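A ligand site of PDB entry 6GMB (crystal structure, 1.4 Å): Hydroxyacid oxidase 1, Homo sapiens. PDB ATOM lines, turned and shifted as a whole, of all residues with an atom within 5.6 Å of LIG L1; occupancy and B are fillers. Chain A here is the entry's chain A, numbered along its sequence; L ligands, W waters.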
ATOM      1  N   TYR A  26       7.272  23.455 -32.089  1.00  0.00           N
ATOM      2  CA  TYR A  26       6.242  23.723 -31.096  1.00  0.00           C
ATOM      3  C   TYR A  26       6.876  23.902 -29.718  1.00  0.00           C
ATOM      4  O   TYR A  26       6.536  24.840 -28.979  1.00  0.00           O
ATOM      5  CB  TYR A  26       5.192  22.611 -31.066  1.00  0.00           C
ATOM      6  CG  TYR A  26       4.348  22.667 -29.812  1.00  0.00           C
ATOM      7  CD1 TYR A  26       3.381  23.651 -29.645  1.00  0.00           C
ATOM      8  CD2 TYR A  26       4.599  21.820 -28.749  1.00  0.00           C
ATOM      9  CE1 TYR A  26       2.666  23.764 -28.474  1.00  0.00           C
ATOM     10  CE2 TYR A  26       3.876  21.905 -27.569  1.00  0.00           C
ATOM     11  CZ  TYR A  26       2.904  22.890 -27.431  1.00  0.00           C
ATOM     12  OH  TYR A  26       2.234  23.006 -26.251  1.00  0.00           O
ATOM     13  N   TYR A  27       7.780  22.995 -29.344  1.00  0.00           N
ATOM     14  CA  TYR A  27       8.394  23.031 -28.024  1.00  0.00           C
ATOM     15  C   TYR A  27       9.369  24.211 -27.892  1.00  0.00           C
ATOM     16  O   TYR A  27       9.417  24.850 -26.838  1.00  0.00           O
ATOM     17  CB  TYR A  27       9.125  21.717 -27.765  1.00  0.00           C
ATOM     18  CG  TYR A  27       8.262  20.498 -27.522  1.00  0.00           C
ATOM     19  CD1 TYR A  27       7.207  20.501 -26.633  1.00  0.00           C
ATOM     20  CD2 TYR A  27       8.593  19.279 -28.124  1.00  0.00           C
ATOM     21  CE1 TYR A  27       6.469  19.352 -26.377  1.00  0.00           C
ATOM     22  CE2 TYR A  27       7.891  18.123 -27.867  1.00  0.00           C
ATOM     23  CZ  TYR A  27       6.818  18.158 -26.996  1.00  0.00           C
ATOM     24  OH  TYR A  27       6.158  16.988 -26.731  1.00  0.00           O
ATOM     25  N   SER A  29       9.531  27.158 -29.652  1.00  0.00           N
ATOM     26  CA  SER A  29       9.122  28.497 -30.065  1.00  0.00           C
ATOM     27  C   SER A  29       8.785  29.412 -28.884  1.00  0.00           C
ATOM     28  O   SER A  29       8.260  28.994 -27.861  1.00  0.00           O
ATOM     29  CB  SER A  29       7.941  28.438 -30.988  1.00  0.00           C
ATOM     30  OG  SER A  29       8.343  28.116 -32.313  1.00  0.00           O
ATOM     31  N   ASN A  40      14.992  35.917 -21.721  1.00  0.00           N
ATOM     32  CA  ASN A  40      14.879  35.053 -20.534  1.00  0.00           C
ATOM     33  C   ASN A  40      16.241  34.439 -20.212  1.00  0.00           C
ATOM     34  O   ASN A  40      16.554  34.239 -19.048  1.00  0.00           O
ATOM     35  CB  ASN A  40      13.837  33.939 -20.698  1.00  0.00           C
ATOM     36  CG  ASN A  40      12.421  34.370 -20.381  1.00  0.00           C
ATOM     37  OD1 ASN A  40      12.204  35.466 -19.849  1.00  0.00           O
ATOM     38  ND2 ASN A  40      11.467  33.509 -20.680  1.00  0.00           N
ATOM     39  N   GLY A  78       8.046  22.166 -14.480  1.00  0.00           N
ATOM     40  CA  GLY A  78       6.918  23.004 -14.852  1.00  0.00           C
ATOM     41  C   GLY A  78       6.029  22.323 -15.877  1.00  0.00           C
ATOM     42  O   GLY A  78       6.436  21.395 -16.569  1.00  0.00           O
ATOM     43  N   ALA A  79       4.800  22.828 -15.985  1.00  0.00           N
ATOM     44  CA  ALA A  79       3.818  22.278 -16.930  1.00  0.00           C
ATOM     45  C   ALA A  79       4.275  22.533 -18.362  1.00  0.00           C
ATOM     46  O   ALA A  79       4.521  23.672 -18.767  1.00  0.00           O
ATOM     47  CB  ALA A  79       2.465  22.914 -16.688  1.00  0.00           C
ATOM     48  N   THR A  80       4.384  21.457 -19.135  1.00  0.00           N
ATOM     49  CA  THR A  80       4.581  21.550 -20.576  1.00  0.00           C
ATOM     50  C   THR A  80       3.600  20.594 -21.238  1.00  0.00           C
ATOM     51  O   THR A  80       3.614  19.410 -20.943  1.00  0.00           O
ATOM     52  CB  THR A  80       6.020  21.256 -21.001  1.00  0.00           C
ATOM     53  OG1 THR A  80       6.449  20.014 -20.438  1.00  0.00           O
ATOM     54  CG2 THR A  80       6.979  22.334 -20.589  1.00  0.00           C
ATOM     55  N   ALA A  81       2.725  21.129 -22.076  1.00  0.00           N
ATOM     56  CA  ALA A  81       1.664  20.365 -22.679  1.00  0.00           C
ATOM     57  C   ALA A  81       2.192  19.236 -23.572  1.00  0.00           C
ATOM     58  O   ALA A  81       3.257  19.320 -24.175  1.00  0.00           O
ATOM     59  CB  ALA A  81       0.792  21.293 -23.485  1.00  0.00           C
ATOM     60  N   MET A 106       4.627  19.616 -11.964  1.00  0.00           N
ATOM     61  CA  MET A 106       3.418  20.353 -12.298  1.00  0.00           C
ATOM     62  C   MET A 106       2.853  19.779 -13.596  1.00  0.00           C
ATOM     63  O   MET A 106       3.509  19.836 -14.619  1.00  0.00           O
ATOM     64  CB  MET A 106       3.747  21.841 -12.471  1.00  0.00           C
ATOM     65  CG  MET A 106       2.532  22.726 -12.585  1.00  0.00           C
ATOM     66  SD  MET A 106       2.884  24.350 -13.287  1.00  0.00           S
ATOM     67  CE  MET A 106       4.182  24.933 -12.187  1.00  0.00           C
ATOM     68  N   SER A 108       0.372  19.665 -16.742  1.00  0.00           N
ATOM     69  CA  SER A 108      -0.430  20.485 -17.640  1.00  0.00           C
ATOM     70  C   SER A 108      -1.885  19.987 -17.713  1.00  0.00           C
ATOM     71  O   SER A 108      -2.120  18.786 -17.847  1.00  0.00           O
ATOM     72  CB  SER A 108       0.175  20.481 -19.007  1.00  0.00           C
ATOM     73  OG  SER A 108      -0.642  21.175 -19.949  1.00  0.00           O
ATOM     74  N   SER A 109      -2.825  20.925 -17.752  1.00  0.00           N
ATOM     75  CA  SER A 109      -4.209  20.601 -18.110  1.00  0.00           C
ATOM     76  C   SER A 109      -4.281  19.983 -19.517  1.00  0.00           C
ATOM     77  O   SER A 109      -5.223  19.237 -19.828  1.00  0.00           O
ATOM     78  CB  SER A 109      -5.098  21.817 -18.063  1.00  0.00           C
ATOM     79  OG  SER A 109      -5.460  22.149 -16.736  1.00  0.00           O
ATOM     80  N   TRP A 110      -3.313  20.327 -20.384  1.00  0.00           N
ATOM     81  CA  TRP A 110      -3.228  19.878 -21.774  1.00  0.00           C
ATOM     82  C   TRP A 110      -2.281  18.680 -21.914  1.00  0.00           C
ATOM     83  O   TRP A 110      -1.706  18.442 -22.977  1.00  0.00           O
ATOM     84  CB  TRP A 110      -2.766  21.033 -22.668  1.00  0.00           C
ATOM     85  CG  TRP A 110      -3.687  22.202 -22.682  1.00  0.00           C
ATOM     86  CD1 TRP A 110      -4.982  22.251 -22.271  1.00  0.00           C
ATOM     87  CD2 TRP A 110      -3.388  23.513 -23.191  1.00  0.00           C
ATOM     88  NE1 TRP A 110      -5.503  23.512 -22.462  1.00  0.00           N
ATOM     89  CE2 TRP A 110      -4.533  24.303 -23.025  1.00  0.00           C
ATOM     90  CE3 TRP A 110      -2.232  24.098 -23.736  1.00  0.00           C
ATOM     91  CZ2 TRP A 110      -4.572  25.645 -23.391  1.00  0.00           C
ATOM     92  CZ3 TRP A 110      -2.279  25.430 -24.109  1.00  0.00           C
ATOM     93  CH2 TRP A 110      -3.431  26.191 -23.921  1.00  0.00           C
ATOM     94  N   GLN A 130      -1.511  22.123 -13.015  1.00  0.00           N
ATOM     95  CA  GLN A 130      -1.655  23.409 -13.689  1.00  0.00           C
ATOM     96  C   GLN A 130      -3.054  23.435 -14.299  1.00  0.00           C
ATOM     97  O   GLN A 130      -3.439  22.515 -15.018  1.00  0.00           O
ATOM     98  CB  GLN A 130      -0.593  23.605 -14.767  1.00  0.00           C
ATOM     99  CG  GLN A 130      -0.791  24.872 -15.584  1.00  0.00           C
ATOM    100  CD  GLN A 130      -1.781  24.746 -16.722  1.00  0.00           C
ATOM    101  OE1 GLN A 130      -2.604  25.654 -16.972  1.00  0.00           O
ATOM    102  NE2 GLN A 130      -1.675  23.665 -17.453  1.00  0.00           N
ATOM    103  N   TYR A 132      -6.069  25.522 -16.436  1.00  0.00           N
ATOM    104  CA  TYR A 132      -6.679  26.517 -17.286  1.00  0.00           C
ATOM    105  C   TYR A 132      -8.157  26.607 -16.941  1.00  0.00           C
ATOM    106  O   TYR A 132      -8.788  25.590 -16.676  1.00  0.00           O
ATOM    107  CB  TYR A 132      -6.514  26.158 -18.771  1.00  0.00           C
ATOM    108  CG  TYR A 132      -5.154  26.432 -19.340  1.00  0.00           C
ATOM    109  CD1 TYR A 132      -4.666  27.725 -19.405  1.00  0.00           C
ATOM    110  CD2 TYR A 132      -4.353  25.403 -19.827  1.00  0.00           C
ATOM    111  CE1 TYR A 132      -3.425  27.998 -19.950  1.00  0.00           C
ATOM    112  CE2 TYR A 132      -3.105  25.664 -20.373  1.00  0.00           C
ATOM    113  CZ  TYR A 132      -2.643  26.967 -20.427  1.00  0.00           C
ATOM    114  OH  TYR A 132      -1.420  27.262 -20.954  1.00  0.00           O
ATOM    115  N   THR A 158      -3.150  29.267 -14.388  1.00  0.00           N
ATOM    116  CA  THR A 158      -2.477  30.074 -15.379  1.00  0.00           C
ATOM    117  C   THR A 158      -3.348  31.292 -15.685  1.00  0.00           C
ATOM    118  O   THR A 158      -4.518  31.144 -16.005  1.00  0.00           O
ATOM    119  CB  THR A 158      -2.161  29.257 -16.633  1.00  0.00           C
ATOM    120  OG1 THR A 158      -1.335  28.172 -16.210  1.00  0.00           O
ATOM    121  CG2 THR A 158      -1.467  30.072 -17.692  1.00  0.00           C
ATOM    122  N   LYS A 236      -0.024  31.695 -11.704  1.00  0.00           N
ATOM    123  CA  LYS A 236       1.070  31.473 -12.641  1.00  0.00           C
ATOM    124  C   LYS A 236       0.954  32.452 -13.820  1.00  0.00           C
ATOM    125  O   LYS A 236      -0.042  32.434 -14.548  1.00  0.00           O
ATOM    126  CB  LYS A 236       1.041  30.013 -13.104  1.00  0.00           C
ATOM    127  CG  LYS A 236       2.024  29.671 -14.207  1.00  0.00           C
ATOM    128  CD  LYS A 236       1.996  28.199 -14.542  1.00  0.00           C
ATOM    129  CE  LYS A 236       3.054  27.772 -15.529  1.00  0.00           C
ATOM    130  NZ  LYS A 236       2.757  28.275 -16.873  1.00  0.00           N
ATOM    131  N   SER A 258       6.348  34.348 -14.210  1.00  0.00           N
ATOM    132  CA  SER A 258       6.407  33.593 -15.433  1.00  0.00           C
ATOM    133  C   SER A 258       5.930  34.478 -16.569  1.00  0.00           C
ATOM    134  O   SER A 258       4.956  35.211 -16.394  1.00  0.00           O
ATOM    135  CB  SER A 258       5.550  32.343 -15.334  1.00  0.00           C
ATOM    136  OG  SER A 258       5.551  31.617 -16.554  1.00  0.00           O
ATOM    137  N   ASN A 259       6.608  34.379 -17.721  1.00  0.00           N
ATOM    138  CA  ASN A 259       6.101  34.934 -18.962  1.00  0.00           C
ATOM    139  C   ASN A 259       5.735  33.787 -19.897  1.00  0.00           C
ATOM    140  O   ASN A 259       5.709  33.948 -21.119  1.00  0.00           O
ATOM    141  CB  ASN A 259       7.065  35.945 -19.576  1.00  0.00           C
ATOM    142  CG  ASN A 259       8.482  35.443 -19.702  1.00  0.00           C
ATOM    143  OD1 ASN A 259       8.698  34.259 -19.965  1.00  0.00           O
ATOM    144  ND2 ASN A 259       9.460  36.334 -19.541  1.00  0.00           N
ATOM    145  N   HIS A 260       5.400  32.624 -19.322  1.00  0.00           N
ATOM    146  CA  HIS A 260       4.912  31.476 -20.089  1.00  0.00           C
ATOM    147  C   HIS A 260       5.983  31.000 -21.072  1.00  0.00           C
ATOM    148  O   HIS A 260       5.699  30.659 -22.205  1.00  0.00           O
ATOM    149  CB  HIS A 260       3.584  31.830 -20.795  1.00  0.00           C
ATOM    150  CG  HIS A 260       2.689  30.675 -21.074  1.00  0.00           C
ATOM    151  ND1 HIS A 260       1.414  30.614 -20.555  1.00  0.00           N
ATOM    152  CD2 HIS A 260       2.822  29.588 -21.873  1.00  0.00           C
ATOM    153  CE1 HIS A 260       0.812  29.519 -20.997  1.00  0.00           C
ATOM    154  NE2 HIS A 260       1.649  28.877 -21.807  1.00  0.00           N
ATOM    155  N   GLY A 261       7.239  30.978 -20.605  1.00  0.00           N
ATOM    156  CA  GLY A 261       8.339  30.567 -21.476  1.00  0.00           C
ATOM    157  C   GLY A 261       8.478  31.461 -22.695  1.00  0.00           C
ATOM    158  O   GLY A 261       8.925  31.024 -23.743  1.00  0.00           O
ATOM    159  N   ARG A 263       6.109  32.657 -24.520  1.00  0.00           N
ATOM    160  CA  ARG A 263       5.225  32.128 -25.564  1.00  0.00           C
ATOM    161  C   ARG A 263       3.905  32.905 -25.680  1.00  0.00           C
ATOM    162  O   ARG A 263       3.100  32.590 -26.565  1.00  0.00           O
ATOM    163  CB  ARG A 263       4.918  30.648 -25.287  1.00  0.00           C
ATOM    164  CG  ARG A 263       6.151  29.765 -25.354  1.00  0.00           C
ATOM    165  CD  ARG A 263       6.000  28.425 -24.667  1.00  0.00           C
ATOM    166  NE  ARG A 263       5.078  27.527 -25.350  1.00  0.00           N
ATOM    167  CZ  ARG A 263       5.447  26.642 -26.271  1.00  0.00           C
ATOM    168  NH1 ARG A 263       6.627  26.768 -26.868  1.00  0.00           N
ATOM    169  NH2 ARG A 263       4.647  25.633 -26.582  1.00  0.00           N
ATOM    170  N   ASP A 291       9.924  30.801 -13.344  1.00  0.00           N
ATOM    171  CA  ASP A 291      10.300  29.984 -14.479  1.00  0.00           C
ATOM    172  C   ASP A 291      10.671  30.921 -15.637  1.00  0.00           C
ATOM    173  O   ASP A 291      10.452  32.129 -15.566  1.00  0.00           O
ATOM    174  CB  ASP A 291       9.230  28.952 -14.822  1.00  0.00           C
ATOM    175  CG  ASP A 291       7.935  29.463 -15.400  1.00  0.00           C
ATOM    176  OD1 ASP A 291       7.925  30.564 -15.955  1.00  0.00           O
ATOM    177  OD2 ASP A 291       6.952  28.709 -15.306  1.00  0.00           O
ATOM    178  N   GLY A 292      11.252  30.335 -16.688  1.00  0.00           N
ATOM    179  CA  GLY A 292      11.634  31.069 -17.874  1.00  0.00           C
ATOM    180  C   GLY A 292      13.130  31.223 -17.995  1.00  0.00           C
ATOM    181  O   GLY A 292      13.731  32.089 -17.337  1.00  0.00           O
ATOM    182  N   GLY A 293      13.736  30.397 -18.841  1.00  0.00           N
ATOM    183  CA  GLY A 293      15.150  30.531 -19.150  1.00  0.00           C
ATOM    184  C   GLY A 293      16.098  29.788 -18.228  1.00  0.00           C
ATOM    185  O   GLY A 293      17.313  29.944 -18.379  1.00  0.00           O
ATOM    186  N   VAL A 294      15.599  28.970 -17.291  1.00  0.00           N
ATOM    187  CA  VAL A 294      16.497  28.231 -16.397  1.00  0.00           C
ATOM    188  C   VAL A 294      17.101  27.063 -17.174  1.00  0.00           C
ATOM    189  O   VAL A 294      16.395  26.165 -17.646  1.00  0.00           O
ATOM    190  CB  VAL A 294      15.757  27.743 -15.145  1.00  0.00           C
ATOM    191  CG1 VAL A 294      16.667  26.866 -14.293  1.00  0.00           C
ATOM    192  CG2 VAL A 294      15.193  28.902 -14.339  1.00  0.00           C
ATOM    193  N   ARG A 295      18.432  27.091 -17.309  1.00  0.00           N
ATOM    194  CA  ARG A 295      19.157  26.100 -18.070  1.00  0.00           C
ATOM    195  C   ARG A 295      20.374  25.569 -17.310  1.00  0.00           C
ATOM    196  O   ARG A 295      20.912  24.539 -17.702  1.00  0.00           O
ATOM    197  CB  ARG A 295      19.663  26.669 -19.393  1.00  0.00           C
ATOM    198  CG  ARG A 295      18.582  27.250 -20.293  1.00  0.00           C
ATOM    199  CD  ARG A 295      17.613  26.227 -20.844  1.00  0.00           C
ATOM    200  NE  ARG A 295      16.565  26.860 -21.647  1.00  0.00           N
ATOM    201  CZ  ARG A 295      15.329  27.115 -21.247  1.00  0.00           C
ATOM    202  NH1 ARG A 295      14.943  26.840 -20.018  1.00  0.00           N
ATOM    203  NH2 ARG A 295      14.465  27.641 -22.115  1.00  0.00           N
ATOM    204  N   PHE A 312      11.050  26.507 -11.664  1.00  0.00           N
ATOM    205  CA  PHE A 312      10.484  25.486 -12.502  1.00  0.00           C
ATOM    206  C   PHE A 312      11.186  25.517 -13.861  1.00  0.00           C
ATOM    207  O   PHE A 312      11.551  26.586 -14.365  1.00  0.00           O
ATOM    208  CB  PHE A 312       8.971  25.671 -12.678  1.00  0.00           C
ATOM    209  CG  PHE A 312       8.195  25.490 -11.397  1.00  0.00           C
ATOM    210  CD1 PHE A 312       8.112  26.502 -10.472  1.00  0.00           C
ATOM    211  CD2 PHE A 312       7.601  24.277 -11.107  1.00  0.00           C
ATOM    212  CE1 PHE A 312       7.437  26.319  -9.271  1.00  0.00           C
ATOM    213  CE2 PHE A 312       6.928  24.088  -9.914  1.00  0.00           C
ATOM    214  CZ  PHE A 312       6.850  25.111  -8.996  1.00  0.00           C
ATOM    215  N   VAL A 313      11.353  24.324 -14.432  1.00  0.00           N
ATOM    216  CA  VAL A 313      11.935  24.166 -15.757  1.00  0.00           C
ATOM    217  C   VAL A 313      10.894  23.557 -16.680  1.00  0.00           C
ATOM    218  O   VAL A 313      10.188  22.607 -16.331  1.00  0.00           O
ATOM    219  CB  VAL A 313      13.234  23.353 -15.760  1.00  0.00           C
ATOM    220  CG1 VAL A 313      14.407  24.159 -15.244  1.00  0.00           C
ATOM    221  CG2 VAL A 313      13.088  22.035 -15.038  1.00  0.00           C
ATOM    222  N   GLY A 314      10.835  24.137 -17.885  1.00  0.00           N
ATOM    223  CA  GLY A 314       9.906  23.711 -18.920  1.00  0.00           C
ATOM    224  C   GLY A 314      10.607  22.900 -19.994  1.00  0.00           C
ATOM    225  O   GLY A 314      10.679  21.669 -19.922  1.00  0.00           O
ATOM    226  N   ARG A 315      11.155  23.597 -20.977  1.00  0.00           N
ATOM    227  CA  ARG A 315      11.713  22.950 -22.154  1.00  0.00           C
ATOM    228  C   ARG A 315      12.766  21.903 -21.813  1.00  0.00           C
ATOM    229  O   ARG A 315      12.794  20.867 -22.481  1.00  0.00           O
ATOM    230  CB  ARG A 315      12.290  23.977 -23.126  1.00  0.00           C
ATOM    231  CG  ARG A 315      11.202  24.812 -23.789  1.00  0.00           C
ATOM    232  CD  ARG A 315      11.777  25.898 -24.651  1.00  0.00           C
ATOM    233  NE  ARG A 315      10.761  26.785 -25.181  1.00  0.00           N
ATOM    234  CZ  ARG A 315      10.396  27.940 -24.640  1.00  0.00           C
ATOM    235  NH1 ARG A 315      10.825  28.299 -23.434  1.00  0.00           N
ATOM    236  NH2 ARG A 315       9.554  28.721 -25.304  1.00  0.00           N
ATOM    237  N   PRO A 316      13.678  22.103 -20.847  1.00  0.00           N
ATOM    238  CA  PRO A 316      14.707  21.078 -20.609  1.00  0.00           C
ATOM    239  C   PRO A 316      14.138  19.672 -20.378  1.00  0.00           C
ATOM    240  O   PRO A 316      14.748  18.681 -20.757  1.00  0.00           O
ATOM    241  CB  PRO A 316      15.432  21.621 -19.378  1.00  0.00           C
ATOM    242  CG  PRO A 316      15.334  23.122 -19.559  1.00  0.00           C
ATOM    243  CD  PRO A 316      13.908  23.318 -20.040  1.00  0.00           C
ATOM    244  N   VAL A 318      11.344  18.405 -21.671  1.00  0.00           N
ATOM    245  CA  VAL A 318      10.911  17.776 -22.919  1.00  0.00           C
ATOM    246  C   VAL A 318      12.151  17.343 -23.725  1.00  0.00           C
ATOM    247  O   VAL A 318      12.092  16.306 -24.387  1.00  0.00           O
ATOM    248  CB  VAL A 318       9.915  18.634 -23.723  1.00  0.00           C
ATOM    249  CG1 VAL A 318       8.622  18.830 -22.958  1.00  0.00           C
ATOM    250  CG2 VAL A 318      10.479  19.970 -24.149  1.00  0.00           C
HETATM  251  N1  LIG L   1       2.181  26.607 -19.171  1.00  0.00           N
HETATM  252  C1  LIG L   1       0.965  26.246 -18.733  1.00  0.00           C
HETATM  253  O1  LIG L   1       0.457  26.883 -17.799  1.00  0.00           O
HETATM  254  N2  LIG L   1       0.288  25.212 -19.284  1.00  0.00           N
HETATM  255  C2  LIG L   1       0.753  24.502 -20.299  1.00  0.00           C
HETATM  256  O2  LIG L   1       0.113  23.567 -20.817  1.00  0.00           O
HETATM  257  C3  LIG L   1       2.053  24.840 -20.844  1.00  0.00           C
HETATM  258  N3  LIG L   1       2.597  24.167 -21.884  1.00  0.00           N
HETATM  259  C4  LIG L   1       3.841  24.487 -22.335  1.00  0.00           C
HETATM  260  C5  LIG L   1       4.408  23.785 -23.387  1.00  0.00           C
HETATM  261  C6  LIG L   1       5.677  24.101 -23.827  1.00  0.00           C
HETATM  262  C7  LIG L   1       6.272  23.317 -24.949  1.00  0.00           C
HETATM  263  C8  LIG L   1       6.420  25.186 -23.184  1.00  0.00           C
HETATM  264  C9  LIG L   1       7.814  25.512 -23.657  1.00  0.00           C
HETATM  265  C10 LIG L   1       5.865  25.885 -22.142  1.00  0.00           C
HETATM  266  C11 LIG L   1       4.588  25.589 -21.692  1.00  0.00           C
HETATM  267  N4  LIG L   1       3.996  26.301 -20.630  1.00  0.00           N
HETATM  268  C12 LIG L   1       2.747  25.941 -20.186  1.00  0.00           C
HETATM  269  C13 LIG L   1       4.754  27.325 -19.919  1.00  0.00           C
HETATM  270  C14 LIG L   1       5.637  26.553 -18.910  1.00  0.00           C
HETATM  271  O3  LIG L   1       4.844  26.093 -17.799  1.00  0.00           O
HETATM  272  C15 LIG L   1       6.749  27.419 -18.327  1.00  0.00           C
HETATM  273  O4  LIG L   1       6.199  28.693 -17.941  1.00  0.00           O
HETATM  274  C16 LIG L   1       7.905  27.632 -19.304  1.00  0.00           C
HETATM  275  O5  LIG L   1       8.191  26.445 -20.049  1.00  0.00           O
HETATM  276  C17 LIG L   1       9.150  28.060 -18.551  1.00  0.00           C
HETATM  277  O6  LIG L   1      10.217  28.432 -19.404  1.00  0.00           O
HETATM  278  P1  LIG L   1      11.366  27.429 -19.934  1.00  0.00           P
HETATM  279  O7  LIG L   1      11.900  26.615 -18.789  1.00  0.00           O
HETATM  280  O8  LIG L   1      10.775  26.560 -21.022  1.00  0.00           O
HETATM  281  O9  LIG L   1      12.379  28.436 -20.440  1.00  0.00           O
HETATM  282  C1  LG2 L   2       1.717  26.270 -24.467  1.00  0.00           C
HETATM  283  C2  LG2 L   2       0.803  25.621 -23.493  1.00  0.00           C
HETATM  284  O1  LG2 L   2       2.401  27.278 -24.117  1.00  0.00           O
HETATM  285  O2  LG2 L   2       1.667  25.695 -25.561  1.00  0.00           O
HETATM  286  O3  LG2 L   2       0.250  26.590 -22.594  1.00  0.00           O
HETATM  287  O   HOH W   1       6.042  26.064 -15.136  1.00  0.00           O
HETATM  288  O   HOH W   2      11.812  30.809 -21.824  1.00  0.00           O
HETATM  289  O   HOH W   3      12.679  27.902 -16.602  1.00  0.00           O
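The backbone NH of Ala 79 sits at hydrogen-bond distance from the side-chain sulfur of Met 106, 3.6 Å away. The side-chain hydroxyl (OG) of Ser 108 sits at hydrogen-bond distance from the backbone NH (N) of Trp 110 (2.8 Å). The side-chain carboxylate (OD1) of Asp 291 is in hydrogen-bond range of the side-chain hydroxyl (OG) of Ser 258, at 2.7 Å. The guanidinium group (NH2) of Arg 315 sits at hydrogen-bond distance from the backbone carbonyl oxygen (O) of Ser 29 (2.9 Å). The guanidinium group (NH1) of Arg 263 is in hydrogen-bond range of the backbone carbonyl oxygen (O) of Tyr 27. The backbone carbonyl oxygen of Tyr 26 sits at hydrogen-bond distance from the guanidinium group of Arg 263 (2.9 Å). The backbone NH (N) of His 260 sits at hydrogen-bond distance from the side-chain hydroxyl (OG) of Ser 258 (2.9 Å). The backbone carbonyl oxygen (O) of Val 313 is in hydrogen-bond range of the backbone NH (N) of Gly 78 (2.9 Å).
N3 of LIG L1 sits close to O3 of LG2 L2 (3.4 Å).
O of Ala 79 is in hydrogen-bond range of O3 of LIG L1. OG of Ser 108 is in hydrogen-bond range of O2 of LIG L1, at 2.7 Å. The side-chain hydroxyl of Thr 158 is in hydrogen-bond range of an oxygen (O1) of LIG L1, 2.7 Å away. The side-chain carboxylate (OD2) of Asp 291 lies within hydrogen-bond range of an oxygen (O4) of LIG L1 (2.7 Å). The guanidinium group of Arg 295 lies within salt-bridge range of an oxygen (O9) of LIG L1 (2.8 Å). NZ of Lys 236 lies within hydrogen-bond range of O1 of LIG L1. The backbone NH (N) of Gly 314 sits at hydrogen-bond distance from an oxygen (O7) of LIG L1, 2.8 Å away. O9 of LIG L1 is in hydrogen-bond range of N of Gly 293 (2.9 Å). An oxygen (O8) of LIG L1 sits at hydrogen-bond distance from the backbone NH (N) of Arg 315 (3.0 Å). The guanidinium group of Arg 315 is in salt-bridge range of an oxygen (O8) of LIG L1 (3.0 Å). The backbone NH of Ala 81 is in hydrogen-bond range of a nitrogen (N3) of LIG L1. NE2 of Gln 130 lies close to N2 of LIG L1 (3.1 Å). The side-chain hydroxyl (OH) of Tyr 132 is in hydrogen-bond range of a nitrogen (N2) of LIG L1 (3.1 Å). OG of Ser 258 sits at hydrogen-bond distance from O4 of LIG L1, 3.3 Å away. N of Gly 292 sits close to O6 of LIG L1, 3.5 Å away. OH of Tyr 132 lies within hydrogen-bond range of O3 of LG2 L2, 2.4 Å away. The guanidinium group (NE) of Arg 263 is in salt-bridge range of an oxygen (O1) of LG2 L2 (3.0 Å). O3 of LG2 L2 sits at hydrogen-bond distance from NE2 of His 260 (2.8 Å). O2 of LG2 L2 sits at hydrogen-bond distance from OH of Tyr 26, 2.8 Å away.
Residues that only touch LIG L1: Tyr 26, Tyr 27, Thr 80, Trp 110, His 260, Gly 261, Arg 263 and Val 313. Of the 32 residues printed, 22 come within 4 Å of LIG L1. Along chain A the residues within 4 Å of LIG L1 span positions 26 to 315.
Water W3 lies within hydrogen-bond range of an oxygen (O7) of LIG L1 (2.7 Å), the backbone NH (N) of Gly 292 (2.8 Å), the backbone carbonyl oxygen (O) of Phe 312 (2.8 Å) and the backbone NH (N) of Val 294 (3.2 Å). Water W2 lies within hydrogen-bond range of O9 of LIG L1 (2.8 Å), ND2 of Asn 40 (3.0 Å), NH1 of Arg 315 (3.1 Å) and O of Gly 261 (3.5 Å). Water W1 bridges OD2 of Asp 291 and O3 of LIG L1.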
